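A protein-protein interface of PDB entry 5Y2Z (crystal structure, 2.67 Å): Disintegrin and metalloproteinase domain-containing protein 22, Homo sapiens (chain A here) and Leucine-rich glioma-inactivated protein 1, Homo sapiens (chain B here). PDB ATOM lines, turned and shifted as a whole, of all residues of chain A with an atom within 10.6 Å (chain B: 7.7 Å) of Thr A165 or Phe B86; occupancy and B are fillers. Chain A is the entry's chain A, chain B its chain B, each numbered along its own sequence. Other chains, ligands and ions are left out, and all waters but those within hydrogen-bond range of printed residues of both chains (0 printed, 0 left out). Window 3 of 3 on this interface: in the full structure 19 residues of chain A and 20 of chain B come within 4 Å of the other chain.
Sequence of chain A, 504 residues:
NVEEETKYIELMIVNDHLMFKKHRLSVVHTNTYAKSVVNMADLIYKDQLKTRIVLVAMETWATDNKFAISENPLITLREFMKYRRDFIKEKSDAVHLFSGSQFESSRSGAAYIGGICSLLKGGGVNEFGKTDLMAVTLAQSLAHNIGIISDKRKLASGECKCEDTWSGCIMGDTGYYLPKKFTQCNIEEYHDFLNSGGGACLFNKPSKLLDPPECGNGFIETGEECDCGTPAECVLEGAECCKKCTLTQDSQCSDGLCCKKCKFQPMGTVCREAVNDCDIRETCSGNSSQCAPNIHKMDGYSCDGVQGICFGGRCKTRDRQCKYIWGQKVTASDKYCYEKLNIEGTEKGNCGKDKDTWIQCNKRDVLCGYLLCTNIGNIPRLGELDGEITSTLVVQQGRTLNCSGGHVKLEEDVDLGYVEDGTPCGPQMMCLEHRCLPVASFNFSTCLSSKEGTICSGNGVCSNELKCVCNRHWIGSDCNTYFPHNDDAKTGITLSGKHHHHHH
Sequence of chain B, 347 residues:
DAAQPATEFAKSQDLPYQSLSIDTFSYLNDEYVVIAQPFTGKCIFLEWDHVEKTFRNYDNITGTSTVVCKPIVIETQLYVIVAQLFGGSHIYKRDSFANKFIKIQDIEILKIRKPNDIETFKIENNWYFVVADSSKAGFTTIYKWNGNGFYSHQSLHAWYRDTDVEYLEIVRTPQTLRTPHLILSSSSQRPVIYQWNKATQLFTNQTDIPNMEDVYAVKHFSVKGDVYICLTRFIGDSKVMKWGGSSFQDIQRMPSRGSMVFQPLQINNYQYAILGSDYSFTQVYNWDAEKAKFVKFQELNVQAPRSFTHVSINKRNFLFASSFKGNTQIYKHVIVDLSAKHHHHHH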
ATOM      1  N   LEU A 155     -22.849 -23.071  -5.725  1.00  0.00           N
ATOM      2  CA  LEU A 155     -22.696 -21.813  -5.013  1.00  0.00           C
ATOM      3  C   LEU A 155     -21.288 -21.278  -5.217  1.00  0.00           C
ATOM      4  O   LEU A 155     -21.097 -20.120  -5.588  1.00  0.00           O
ATOM      5  CB  LEU A 155     -22.983 -21.991  -3.523  1.00  0.00           C
ATOM      6  CG  LEU A 155     -24.447 -21.988  -3.087  1.00  0.00           C
ATOM      7  CD1 LEU A 155     -24.533 -22.225  -1.590  1.00  0.00           C
ATOM      8  CD2 LEU A 155     -25.126 -20.686  -3.472  1.00  0.00           C
ATOM      9  N   CYS A 160     -25.357 -21.095  -9.099  1.00  0.00           N
ATOM     10  CA  CYS A 160     -26.582 -20.704  -8.418  1.00  0.00           C
ATOM     11  C   CYS A 160     -26.304 -19.544  -7.474  1.00  0.00           C
ATOM     12  O   CYS A 160     -25.440 -19.637  -6.604  1.00  0.00           O
ATOM     13  CB  CYS A 160     -27.182 -21.885  -7.647  1.00  0.00           C
ATOM     14  SG  CYS A 160     -27.827 -23.230  -8.683  1.00  0.00           S
ATOM     15  N   LYS A 161     -27.030 -18.446  -7.654  1.00  0.00           N
ATOM     16  CA  LYS A 161     -26.867 -17.284  -6.790  1.00  0.00           C
ATOM     17  C   LYS A 161     -28.216 -16.675  -6.430  1.00  0.00           C
ATOM     18  O   LYS A 161     -29.156 -16.713  -7.225  1.00  0.00           O
ATOM     19  CB  LYS A 161     -25.978 -16.229  -7.457  1.00  0.00           C
ATOM     20  CG  LYS A 161     -24.493 -16.583  -7.527  1.00  0.00           C
ATOM     21  CD  LYS A 161     -23.682 -15.897  -6.427  1.00  0.00           C
ATOM     22  CE  LYS A 161     -23.798 -16.626  -5.096  1.00  0.00           C
ATOM     23  NZ  LYS A 161     -23.367 -18.050  -5.212  1.00  0.00           N
ATOM     24  N   CYS A 162     -28.309 -16.126  -5.224  1.00  0.00           N
ATOM     25  CA  CYS A 162     -29.513 -15.433  -4.792  1.00  0.00           C
ATOM     26  C   CYS A 162     -29.540 -14.011  -5.353  1.00  0.00           C
ATOM     27  O   CYS A 162     -28.658 -13.206  -5.062  1.00  0.00           O
ATOM     28  CB  CYS A 162     -29.603 -15.408  -3.267  1.00  0.00           C
ATOM     29  SG  CYS A 162     -31.072 -14.583  -2.643  1.00  0.00           S
ATOM     30  N   GLU A 163     -30.552 -13.711  -6.162  1.00  0.00           N
ATOM     31  CA  GLU A 163     -30.648 -12.410  -6.815  1.00  0.00           C
ATOM     32  C   GLU A 163     -31.113 -11.304  -5.865  1.00  0.00           C
ATOM     33  O   GLU A 163     -31.043 -10.119  -6.200  1.00  0.00           O
ATOM     34  CB  GLU A 163     -31.583 -12.494  -8.029  1.00  0.00           C
ATOM     35  CG  GLU A 163     -31.028 -13.330  -9.184  1.00  0.00           C
ATOM     36  CD  GLU A 163     -32.074 -13.661 -10.239  1.00  0.00           C
ATOM     37  OE1 GLU A 163     -33.177 -13.076 -10.191  1.00  0.00           O
ATOM     38  OE2 GLU A 163     -31.792 -14.509 -11.115  1.00  0.00           O
ATOM     39  N   ASP A 164     -31.586 -11.689  -4.682  1.00  0.00           N
ATOM     40  CA  ASP A 164     -32.032 -10.717  -3.686  1.00  0.00           C
ATOM     41  C   ASP A 164     -30.847 -10.232  -2.854  1.00  0.00           C
ATOM     42  O   ASP A 164     -30.323 -10.957  -2.011  1.00  0.00           O
ATOM     43  CB  ASP A 164     -33.113 -11.324  -2.787  1.00  0.00           C
ATOM     44  CG  ASP A 164     -33.819 -10.286  -1.925  1.00  0.00           C
ATOM     45  OD1 ASP A 164     -33.183  -9.291  -1.524  1.00  0.00           O
ATOM     46  OD2 ASP A 164     -35.028 -10.459  -1.658  1.00  0.00           O
ATOM     47  N   THR A 165     -30.457  -8.983  -3.084  1.00  0.00           N
ATOM     48  CA  THR A 165     -29.255  -8.418  -2.483  1.00  0.00           C
ATOM     49  C   THR A 165     -29.471  -8.044  -1.022  1.00  0.00           C
ATOM     50  O   THR A 165     -28.546  -8.090  -0.212  1.00  0.00           O
ATOM     51  CB  THR A 165     -28.787  -7.173  -3.252  1.00  0.00           C
ATOM     52  OG1 THR A 165     -28.772  -7.454  -4.656  1.00  0.00           O
ATOM     53  CG2 THR A 165     -27.399  -6.763  -2.810  1.00  0.00           C
ATOM     54  N   TRP A 166     -30.703  -7.671  -0.691  1.00  0.00           N
ATOM     55  CA  TRP A 166     -30.998  -7.121   0.622  1.00  0.00           C
ATOM     56  C   TRP A 166     -31.511  -8.168   1.603  1.00  0.00           C
ATOM     57  O   TRP A 166     -30.946  -8.346   2.683  1.00  0.00           O
ATOM     58  CB  TRP A 166     -32.022  -5.993   0.497  1.00  0.00           C
ATOM     59  CG  TRP A 166     -32.429  -5.423   1.813  1.00  0.00           C
ATOM     60  CD1 TRP A 166     -33.574  -5.692   2.503  1.00  0.00           C
ATOM     61  CD2 TRP A 166     -31.688  -4.493   2.608  1.00  0.00           C
ATOM     62  NE1 TRP A 166     -33.596  -4.981   3.677  1.00  0.00           N
ATOM     63  CE2 TRP A 166     -32.449  -4.237   3.766  1.00  0.00           C
ATOM     64  CE3 TRP A 166     -30.456  -3.850   2.453  1.00  0.00           C
ATOM     65  CZ2 TRP A 166     -32.018  -3.369   4.764  1.00  0.00           C
ATOM     66  CZ3 TRP A 166     -30.029  -2.985   3.447  1.00  0.00           C
ATOM     67  CH2 TRP A 166     -30.808  -2.753   4.586  1.00  0.00           C
ATOM     68  N   SER A 167     -32.576  -8.870   1.230  1.00  0.00           N
ATOM     69  CA  SER A 167     -33.201  -9.805   2.156  1.00  0.00           C
ATOM     70  C   SER A 167     -32.590 -11.193   2.032  1.00  0.00           C
ATOM     71  O   SER A 167     -32.730 -12.023   2.928  1.00  0.00           O
ATOM     72  CB  SER A 167     -34.712  -9.874   1.913  1.00  0.00           C
ATOM     73  OG  SER A 167     -35.315  -8.597   2.027  1.00  0.00           O
ATOM     74  N   GLY A 168     -31.902 -11.439   0.924  1.00  0.00           N
ATOM     75  CA  GLY A 168     -31.281 -12.729   0.695  1.00  0.00           C
ATOM     76  C   GLY A 168     -32.300 -13.828   0.479  1.00  0.00           C
ATOM     77  O   GLY A 168     -33.479 -13.552   0.253  1.00  0.00           O
ATOM     78  N   CYS A 169     -31.859 -15.079   0.589  1.00  0.00           N
ATOM     79  CA  CYS A 169     -32.751 -16.214   0.364  1.00  0.00           C
ATOM     80  C   CYS A 169     -32.840 -17.156   1.569  1.00  0.00           C
ATOM     81  O   CYS A 169     -31.999 -17.130   2.469  1.00  0.00           O
ATOM     82  CB  CYS A 169     -32.302 -16.995  -0.872  1.00  0.00           C
ATOM     83  SG  CYS A 169     -32.431 -16.076  -2.427  1.00  0.00           S
ATOM     84  N   ASP A 173     -27.814 -17.888   5.359  1.00  0.00           N
ATOM     85  CA  ASP A 173     -27.740 -17.483   6.760  1.00  0.00           C
ATOM     86  C   ASP A 173     -28.756 -16.386   7.047  1.00  0.00           C
ATOM     87  O   ASP A 173     -28.820 -15.384   6.336  1.00  0.00           O
ATOM     88  CB  ASP A 173     -26.333 -17.001   7.120  1.00  0.00           C
ATOM     89  CG  ASP A 173     -25.275 -18.058   6.888  1.00  0.00           C
ATOM     90  OD1 ASP A 173     -25.593 -19.260   7.014  1.00  0.00           O
ATOM     91  OD2 ASP A 173     -24.120 -17.683   6.592  1.00  0.00           O
ATOM     92  N   TYR A 177     -33.064  -8.807   8.825  1.00  0.00           N
ATOM     93  CA  TYR A 177     -33.899  -8.686   7.639  1.00  0.00           C
ATOM     94  C   TYR A 177     -34.126 -10.058   6.998  1.00  0.00           C
ATOM     95  O   TYR A 177     -33.242 -10.602   6.333  1.00  0.00           O
ATOM     96  CB  TYR A 177     -33.273  -7.710   6.649  1.00  0.00           C
ATOM     97  CG  TYR A 177     -33.131  -6.312   7.205  1.00  0.00           C
ATOM     98  CD1 TYR A 177     -34.218  -5.454   7.267  1.00  0.00           C
ATOM     99  CD2 TYR A 177     -31.906  -5.845   7.661  1.00  0.00           C
ATOM    100  CE1 TYR A 177     -34.094  -4.177   7.775  1.00  0.00           C
ATOM    101  CE2 TYR A 177     -31.769  -4.564   8.168  1.00  0.00           C
ATOM    102  CZ  TYR A 177     -32.866  -3.735   8.223  1.00  0.00           C
ATOM    103  OH  TYR A 177     -32.741  -2.458   8.730  1.00  0.00           O
ATOM    104  N   LEU A 178     -35.327 -10.595   7.190  1.00  0.00           N
ATOM    105  CA  LEU A 178     -35.642 -11.974   6.823  1.00  0.00           C
ATOM    106  C   LEU A 178     -35.837 -12.181   5.331  1.00  0.00           C
ATOM    107  O   LEU A 178     -36.388 -11.324   4.644  1.00  0.00           O
ATOM    108  CB  LEU A 178     -36.902 -12.434   7.557  1.00  0.00           C
ATOM    109  CG  LEU A 178     -36.877 -12.309   9.080  1.00  0.00           C
ATOM    110  CD1 LEU A 178     -38.191 -12.778   9.667  1.00  0.00           C
ATOM    111  CD2 LEU A 178     -35.715 -13.099   9.652  1.00  0.00           C
ATOM    112  N   PRO A 179     -35.390 -13.340   4.824  1.00  0.00           N
ATOM    113  CA  PRO A 179     -35.587 -13.713   3.421  1.00  0.00           C
ATOM    114  C   PRO A 179     -37.038 -14.089   3.153  1.00  0.00           C
ATOM    115  O   PRO A 179     -37.782 -14.389   4.087  1.00  0.00           O
ATOM    116  CB  PRO A 179     -34.671 -14.919   3.249  1.00  0.00           C
ATOM    117  CG  PRO A 179     -34.633 -15.537   4.603  1.00  0.00           C
ATOM    118  CD  PRO A 179     -34.708 -14.403   5.583  1.00  0.00           C
ATOM    119  N   LYS A 180     -37.423 -14.103   1.883  1.00  0.00           N
ATOM    120  CA  LYS A 180     -38.802 -14.381   1.514  1.00  0.00           C
ATOM    121  C   LYS A 180     -38.876 -15.379   0.358  1.00  0.00           C
ATOM    122  O   LYS A 180     -39.926 -15.968   0.099  1.00  0.00           O
ATOM    123  CB  LYS A 180     -39.512 -13.071   1.140  1.00  0.00           C
ATOM    124  CG  LYS A 180     -41.019 -13.178   0.992  1.00  0.00           C
ATOM    125  CD  LYS A 180     -41.622 -11.873   0.491  1.00  0.00           C
ATOM    126  CE  LYS A 180     -43.124 -12.007   0.268  1.00  0.00           C
ATOM    127  NZ  LYS A 180     -43.742 -10.751  -0.241  1.00  0.00           N
ATOM    128  N   LYS A 181     -37.752 -15.584  -0.322  1.00  0.00           N
ATOM    129  CA  LYS A 181     -37.759 -16.343  -1.568  1.00  0.00           C
ATOM    130  C   LYS A 181     -36.725 -17.467  -1.607  1.00  0.00           C
ATOM    131  O   LYS A 181     -35.626 -17.341  -1.062  1.00  0.00           O
ATOM    132  CB  LYS A 181     -37.520 -15.406  -2.756  1.00  0.00           C
ATOM    133  CG  LYS A 181     -38.589 -14.345  -2.950  1.00  0.00           C
ATOM    134  CD  LYS A 181     -38.280 -13.466  -4.155  1.00  0.00           C
ATOM    135  CE  LYS A 181     -39.349 -12.396  -4.355  1.00  0.00           C
ATOM    136  NZ  LYS A 181     -39.307 -11.351  -3.288  1.00  0.00           N
ATOM    137  N   THR A 183     -34.290 -19.712  -4.213  1.00  0.00           N
ATOM    138  CA  THR A 183     -33.625 -19.475  -5.487  1.00  0.00           C
ATOM    139  C   THR A 183     -34.232 -20.383  -6.551  1.00  0.00           C
ATOM    140  O   THR A 183     -34.927 -21.346  -6.226  1.00  0.00           O
ATOM    141  CB  THR A 183     -32.108 -19.726  -5.406  1.00  0.00           C
ATOM    142  OG1 THR A 183     -31.864 -21.108  -5.119  1.00  0.00           O
ATOM    143  CG2 THR A 183     -31.482 -18.874  -4.323  1.00  0.00           C
ATOM    144  N   PRO B  38     -29.722   2.092   1.921  1.00  0.00           N
ATOM    145  CA  PRO B  38     -29.844   0.635   1.844  1.00  0.00           C
ATOM    146  C   PRO B  38     -30.096   0.148   0.427  1.00  0.00           C
ATOM    147  O   PRO B  38     -29.450  -0.784  -0.048  1.00  0.00           O
ATOM    148  CB  PRO B  38     -31.055   0.334   2.739  1.00  0.00           C
ATOM    149  CG  PRO B  38     -31.233   1.548   3.579  1.00  0.00           C
ATOM    150  CD  PRO B  38     -30.801   2.689   2.722  1.00  0.00           C
ATOM    151  N   PHE B  39     -31.037   0.799  -0.242  1.00  0.00           N
ATOM    152  CA  PHE B  39     -31.591   0.280  -1.480  1.00  0.00           C
ATOM    153  C   PHE B  39     -30.772   0.631  -2.722  1.00  0.00           C
ATOM    154  O   PHE B  39     -30.776  -0.102  -3.710  1.00  0.00           O
ATOM    155  CB  PHE B  39     -33.013   0.816  -1.618  1.00  0.00           C
ATOM    156  CG  PHE B  39     -33.918   0.394  -0.494  1.00  0.00           C
ATOM    157  CD1 PHE B  39     -33.747  -0.835   0.129  1.00  0.00           C
ATOM    158  CD2 PHE B  39     -34.903   1.249  -0.025  1.00  0.00           C
ATOM    159  CE1 PHE B  39     -34.564  -1.217   1.178  1.00  0.00           C
ATOM    160  CE2 PHE B  39     -35.723   0.877   1.022  1.00  0.00           C
ATOM    161  CZ  PHE B  39     -35.555  -0.360   1.626  1.00  0.00           C
ATOM    162  N   GLY B  63     -21.578   0.781  -1.818  1.00  0.00           N
ATOM    163  CA  GLY B  63     -21.563  -0.549  -1.227  1.00  0.00           C
ATOM    164  C   GLY B  63     -22.952  -1.144  -1.359  1.00  0.00           C
ATOM    165  O   GLY B  63     -23.922  -0.546  -0.914  1.00  0.00           O
ATOM    166  N   THR B  64     -23.044  -2.347  -1.912  1.00  0.00           N
ATOM    167  CA  THR B  64     -24.322  -2.903  -2.359  1.00  0.00           C
ATOM    168  C   THR B  64     -25.480  -2.930  -1.348  1.00  0.00           C
ATOM    169  O   THR B  64     -26.625  -2.661  -1.722  1.00  0.00           O
ATOM    170  CB  THR B  64     -24.115  -4.337  -2.862  1.00  0.00           C
ATOM    171  OG1 THR B  64     -23.594  -5.143  -1.799  1.00  0.00           O
ATOM    172  CG2 THR B  64     -23.133  -4.349  -4.019  1.00  0.00           C
ATOM    173  N   SER B  65     -25.208  -3.232  -0.085  1.00  0.00           N
ATOM    174  CA  SER B  65     -26.284  -3.243   0.911  1.00  0.00           C
ATOM    175  C   SER B  65     -25.842  -2.642   2.229  1.00  0.00           C
ATOM    176  O   SER B  65     -25.749  -3.352   3.232  1.00  0.00           O
ATOM    177  CB  SER B  65     -26.789  -4.666   1.144  1.00  0.00           C
ATOM    178  OG  SER B  65     -27.405  -5.185  -0.017  1.00  0.00           O
ATOM    179  N   THR B  66     -25.607  -1.333   2.240  1.00  0.00           N
ATOM    180  CA  THR B  66     -25.102  -0.682   3.441  1.00  0.00           C
ATOM    181  C   THR B  66     -26.191  -0.516   4.491  1.00  0.00           C
ATOM    182  O   THR B  66     -27.321  -0.145   4.182  1.00  0.00           O
ATOM    183  CB  THR B  66     -24.503   0.704   3.121  1.00  0.00           C
ATOM    184  OG1 THR B  66     -25.504   1.547   2.544  1.00  0.00           O
ATOM    185  CG2 THR B  66     -23.333   0.569   2.162  1.00  0.00           C
ATOM    186  N   VAL B  67     -25.824  -0.779   5.740  1.00  0.00           N
ATOM    187  CA  VAL B  67     -26.737  -0.657   6.868  1.00  0.00           C
ATOM    188  C   VAL B  67     -26.292   0.466   7.786  1.00  0.00           C
ATOM    189  O   VAL B  67     -27.108   1.251   8.270  1.00  0.00           O
ATOM    190  CB  VAL B  67     -26.822  -1.967   7.668  1.00  0.00           C
ATOM    191  CG1 VAL B  67     -27.725  -1.795   8.885  1.00  0.00           C
ATOM    192  CG2 VAL B  67     -27.326  -3.080   6.783  1.00  0.00           C
ATOM    193  N   VAL B  82     -18.049   0.645   6.951  1.00  0.00           N
ATOM    194  CA  VAL B  82     -19.221   0.399   6.124  1.00  0.00           C
ATOM    195  C   VAL B  82     -19.744  -1.022   6.298  1.00  0.00           C
ATOM    196  O   VAL B  82     -19.177  -1.975   5.764  1.00  0.00           O
ATOM    197  CB  VAL B  82     -18.911   0.650   4.642  1.00  0.00           C
ATOM    198  CG1 VAL B  82     -20.140   0.380   3.796  1.00  0.00           C
ATOM    199  CG2 VAL B  82     -18.435   2.077   4.447  1.00  0.00           C
ATOM    200  N   ALA B  83     -20.830  -1.152   7.051  1.00  0.00           N
ATOM    201  CA  ALA B  83     -21.467  -2.444   7.271  1.00  0.00           C
ATOM    202  C   ALA B  83     -22.407  -2.792   6.121  1.00  0.00           C
ATOM    203  O   ALA B  83     -23.337  -2.044   5.827  1.00  0.00           O
ATOM    204  CB  ALA B  83     -22.223  -2.439   8.592  1.00  0.00           C
ATOM    205  N   GLN B  84     -22.163  -3.925   5.471  1.00  0.00           N
ATOM    206  CA  GLN B  84     -22.988  -4.341   4.341  1.00  0.00           C
ATOM    207  C   GLN B  84     -23.590  -5.723   4.565  1.00  0.00           C
ATOM    208  O   GLN B  84     -22.966  -6.588   5.177  1.00  0.00           O
ATOM    209  CB  GLN B  84     -22.177  -4.327   3.042  1.00  0.00           C
ATOM    210  CG  GLN B  84     -21.579  -2.971   2.707  1.00  0.00           C
ATOM    211  CD  GLN B  84     -20.721  -2.991   1.454  1.00  0.00           C
ATOM    212  OE1 GLN B  84     -19.949  -2.067   1.206  1.00  0.00           O
ATOM    213  NE2 GLN B  84     -20.855  -4.043   0.656  1.00  0.00           N
ATOM    214  N   LEU B  85     -24.816  -5.919   4.091  1.00  0.00           N
ATOM    215  CA  LEU B  85     -25.467  -7.223   4.187  1.00  0.00           C
ATOM    216  C   LEU B  85     -25.020  -8.125   3.041  1.00  0.00           C
ATOM    217  O   LEU B  85     -25.139  -9.347   3.108  1.00  0.00           O
ATOM    218  CB  LEU B  85     -26.987  -7.063   4.181  1.00  0.00           C
ATOM    219  CG  LEU B  85     -27.522  -6.349   5.423  1.00  0.00           C
ATOM    220  CD1 LEU B  85     -29.040  -6.263   5.421  1.00  0.00           C
ATOM    221  CD2 LEU B  85     -27.005  -7.017   6.694  1.00  0.00           C
ATOM    222  N   PHE B  86     -24.503  -7.504   1.988  1.00  0.00           N
ATOM    223  CA  PHE B  86     -24.014  -8.228   0.828  1.00  0.00           C
ATOM    224  C   PHE B  86     -22.557  -7.902   0.537  1.00  0.00           C
ATOM    225  O   PHE B  86     -22.106  -6.762   0.667  1.00  0.00           O
ATOM    226  CB  PHE B  86     -24.885  -7.916  -0.393  1.00  0.00           C
ATOM    227  CG  PHE B  86     -24.570  -8.747  -1.603  1.00  0.00           C
ATOM    228  CD1 PHE B  86     -25.012 -10.056  -1.702  1.00  0.00           C
ATOM    229  CD2 PHE B  86     -23.837  -8.210  -2.648  1.00  0.00           C
ATOM    230  CE1 PHE B  86     -24.723 -10.817  -2.824  1.00  0.00           C
ATOM    231  CE2 PHE B  86     -23.547  -8.962  -3.770  1.00  0.00           C
ATOM    232  CZ  PHE B  86     -23.989 -10.268  -3.860  1.00  0.00           C
ATOM    233  N   GLY B  87     -21.821  -8.926   0.116  1.00  0.00           N
ATOM    234  CA  GLY B  87     -20.430  -8.766  -0.279  1.00  0.00           C
ATOM    235  C   GLY B  87     -19.452  -8.547   0.862  1.00  0.00           C
ATOM    236  O   GLY B  87     -18.238  -8.572   0.647  1.00  0.00           O
ATOM    237  N   GLY B  88     -19.949  -8.312   2.069  1.00  0.00           N
ATOM    238  CA  GLY B  88     -19.085  -8.142   3.237  1.00  0.00           C
ATOM    239  C   GLY B  88     -18.865  -6.698   3.663  1.00  0.00           C
ATOM    240  O   GLY B  88     -19.230  -5.782   2.932  1.00  0.00           O
ATOM    241  N   SER B  89     -18.283  -6.471   4.847  1.00  0.00           N
ATOM    242  CA  SER B  89     -18.060  -5.095   5.321  1.00  0.00           C
ATOM    243  C   SER B  89     -16.633  -4.603   5.036  1.00  0.00           C
ATOM    244  O   SER B  89     -15.686  -5.392   5.003  1.00  0.00           O
ATOM    245  CB  SER B  89     -18.358  -4.977   6.820  1.00  0.00           C
ATOM    246  OG  SER B  89     -19.719  -5.266   7.079  1.00  0.00           O
ATOM    247  N   HIS B  90     -16.485  -3.297   4.829  1.00  0.00           N
ATOM    248  CA  HIS B  90     -15.180  -2.728   4.500  1.00  0.00           C
ATOM    249  C   HIS B  90     -14.861  -1.476   5.289  1.00  0.00           C
ATOM    250  O   HIS B  90     -15.748  -0.859   5.866  1.00  0.00           O
ATOM    251  CB  HIS B  90     -15.096  -2.402   3.019  1.00  0.00           C
ATOM    252  CG  HIS B  90     -15.662  -3.465   2.142  1.00  0.00           C
ATOM    253  ND1 HIS B  90     -14.932  -4.565   1.752  1.00  0.00           N
ATOM    254  CD2 HIS B  90     -16.881  -3.594   1.569  1.00  0.00           C
ATOM    255  CE1 HIS B  90     -15.678  -5.332   0.979  1.00  0.00           C
ATOM    256  NE2 HIS B  90     -16.861  -4.760   0.843  1.00  0.00           N
ATOM    257  N   ILE B 109     -15.841 -11.854   5.477  1.00  0.00           N
ATOM    258  CA  ILE B 109     -17.271 -12.087   5.326  1.00  0.00           C
ATOM    259  C   ILE B 109     -17.841 -13.187   6.234  1.00  0.00           C
ATOM    260  O   ILE B 109     -19.045 -13.215   6.481  1.00  0.00           O
ATOM    261  CB  ILE B 109     -17.615 -12.429   3.869  1.00  0.00           C
ATOM    262  CG1 ILE B 109     -16.822 -13.646   3.397  1.00  0.00           C
ATOM    263  CG2 ILE B 109     -17.321 -11.245   2.968  1.00  0.00           C
ATOM    264  CD1 ILE B 109     -17.078 -13.994   1.950  1.00  0.00           C
ATOM    265  N   ARG B 113     -21.409 -11.366   9.173  1.00  0.00           N
ATOM    266  CA  ARG B 113     -22.271 -11.736   8.053  1.00  0.00           C
ATOM    267  C   ARG B 113     -23.521 -10.865   7.922  1.00  0.00           C
ATOM    268  O   ARG B 113     -23.848 -10.395   6.831  1.00  0.00           O
ATOM    269  CB  ARG B 113     -22.683 -13.204   8.183  1.00  0.00           C
ATOM    270  CG  ARG B 113     -21.527 -14.129   8.525  1.00  0.00           C
ATOM    271  CD  ARG B 113     -21.926 -15.594   8.418  1.00  0.00           C
ATOM    272  NE  ARG B 113     -20.820 -16.473   8.788  1.00  0.00           N
ATOM    273  CZ  ARG B 113     -20.798 -17.783   8.563  1.00  0.00           C
ATOM    274  NH1 ARG B 113     -21.824 -18.371   7.963  1.00  0.00           N
ATOM    275  NH2 ARG B 113     -19.749 -18.503   8.936  1.00  0.00           N
ATOM    276  N   LYS B 114     -24.226 -10.662   9.032  1.00  0.00           N
ATOM    277  CA  LYS B 114     -25.431  -9.842   9.024  1.00  0.00           C
ATOM    278  C   LYS B 114     -25.372  -8.707  10.050  1.00  0.00           C
ATOM    279  O   LYS B 114     -26.067  -8.745  11.072  1.00  0.00           O
ATOM    280  CB  LYS B 114     -26.661 -10.711   9.284  1.00  0.00           C
ATOM    281  CG  LYS B 114     -27.631 -10.800   8.109  1.00  0.00           C
ATOM    282  CD  LYS B 114     -27.178 -11.784   7.040  1.00  0.00           C
ATOM    283  CE  LYS B 114     -28.188 -11.837   5.903  1.00  0.00           C
ATOM    284  NZ  LYS B 114     -27.845 -12.845   4.871  1.00  0.00           N
ATOM    285  N   PRO B 115     -24.560  -7.674   9.766  1.00  0.00           N
ATOM    286  CA  PRO B 115     -24.423  -6.537  10.682  1.00  0.00           C
ATOM    287  C   PRO B 115     -25.706  -5.726  10.763  1.00  0.00           C
ATOM    288  O   PRO B 115     -26.462  -5.684   9.797  1.00  0.00           O
ATOM    289  CB  PRO B 115     -23.288  -5.722  10.058  1.00  0.00           C
ATOM    290  CG  PRO B 115     -23.346  -6.051   8.613  1.00  0.00           C
ATOM    291  CD  PRO B 115     -23.768  -7.491   8.538  1.00  0.00           C
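Of the 20 printed residues of chain B, 7 touch a printed residue of chain A.
Printed residues of chain B that touch a printed residue of chain A: Pro B38, Ser B65, Thr B66, Leu B85, Phe B86, Arg B113 and Lys B114.
Hydrophobic or aromatic side chains of chain B within 4 Å of the printed part of chain A: Pro B38, Leu B85 and Phe B86.
Among the printed residues, 9 pairs touch across the chains.
Among the printed residues, Asp or Glu carboxylates within 4 Å of a Lys or Arg side-chain nitrogen of the other chain: Asp A173 with Arg B113.
The side-chain hydroxyl (OG) of Ser B65 lies within hydrogen-bond range of the backbone carbonyl oxygen (O) of Thr A165, at 3.1 Å.
The guanidinium group of Arg B113 is in salt-bridge range of the side-chain carboxylate of Asp A173 (2.8 Å).
The side-chain amino group (NZ) of Lys B114 is in hydrogen-bond range of the backbone carbonyl oxygen (O) of Asp A173 (3.1 Å).
The backbone NH of Trp A166 lies within hydrogen-bond range of the side-chain carboxylate of Asp A164.
The backbone carbonyl oxygen (O) of Phe B86 lies close to the side-chain hydroxyl (OG1) of Thr B64.
O of Ser B65 lies within hydrogen-bond range of N of Leu B85, at 2.9 Å.
The backbone carbonyl oxygen of Phe B86 lies within hydrogen-bond range of the side-chain amide nitrogen of Gln B84 (3.0 Å).
The side-chain sulfur (SG) of Cys A169 is disulfide-bonded to the side-chain sulfur (SG) of Cys A162 (2.0 Å).
Among the printed residues, pairs that only touch across the chains: Trp A166 with Pro B38, Thr A165 with Phe B86, Tyr A177 with Leu B85, Trp A166 with Leu B85, Trp A166 with Ser B65 and Trp A166 with Thr B66.
Of chain B, only Ser B65 and Phe B86 come within 4 Å of Thr A165.
Phe B86 touches one residue of chain A.
No residue of chain A comes within 4 Å of Thr B64.
Of chain A, only Trp A166 (3.9 Å) and Tyr A177 (3.7 Å) come within 4 Å of Leu B85.
Gly B87 touches none of the printed residues of chain A.
No residue of chain A comes within 4 Å of Gly B88.
Of the printed residues of chain A, Pro B38 touches Trp A166.
Of the printed residues of chain A, Lys B114 touches Asp A173 (3.1 Å).
Printed residues of chain B within 4 Å of Tyr A177: Leu B85 (3.7 Å).
Of the printed residues of chain A, Arg B113 touches Asp A173.
Printed residues of chain B within 4 Å of Asp A173: Arg B113 (2.8 Å) and Lys B114 (3.1 Å).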
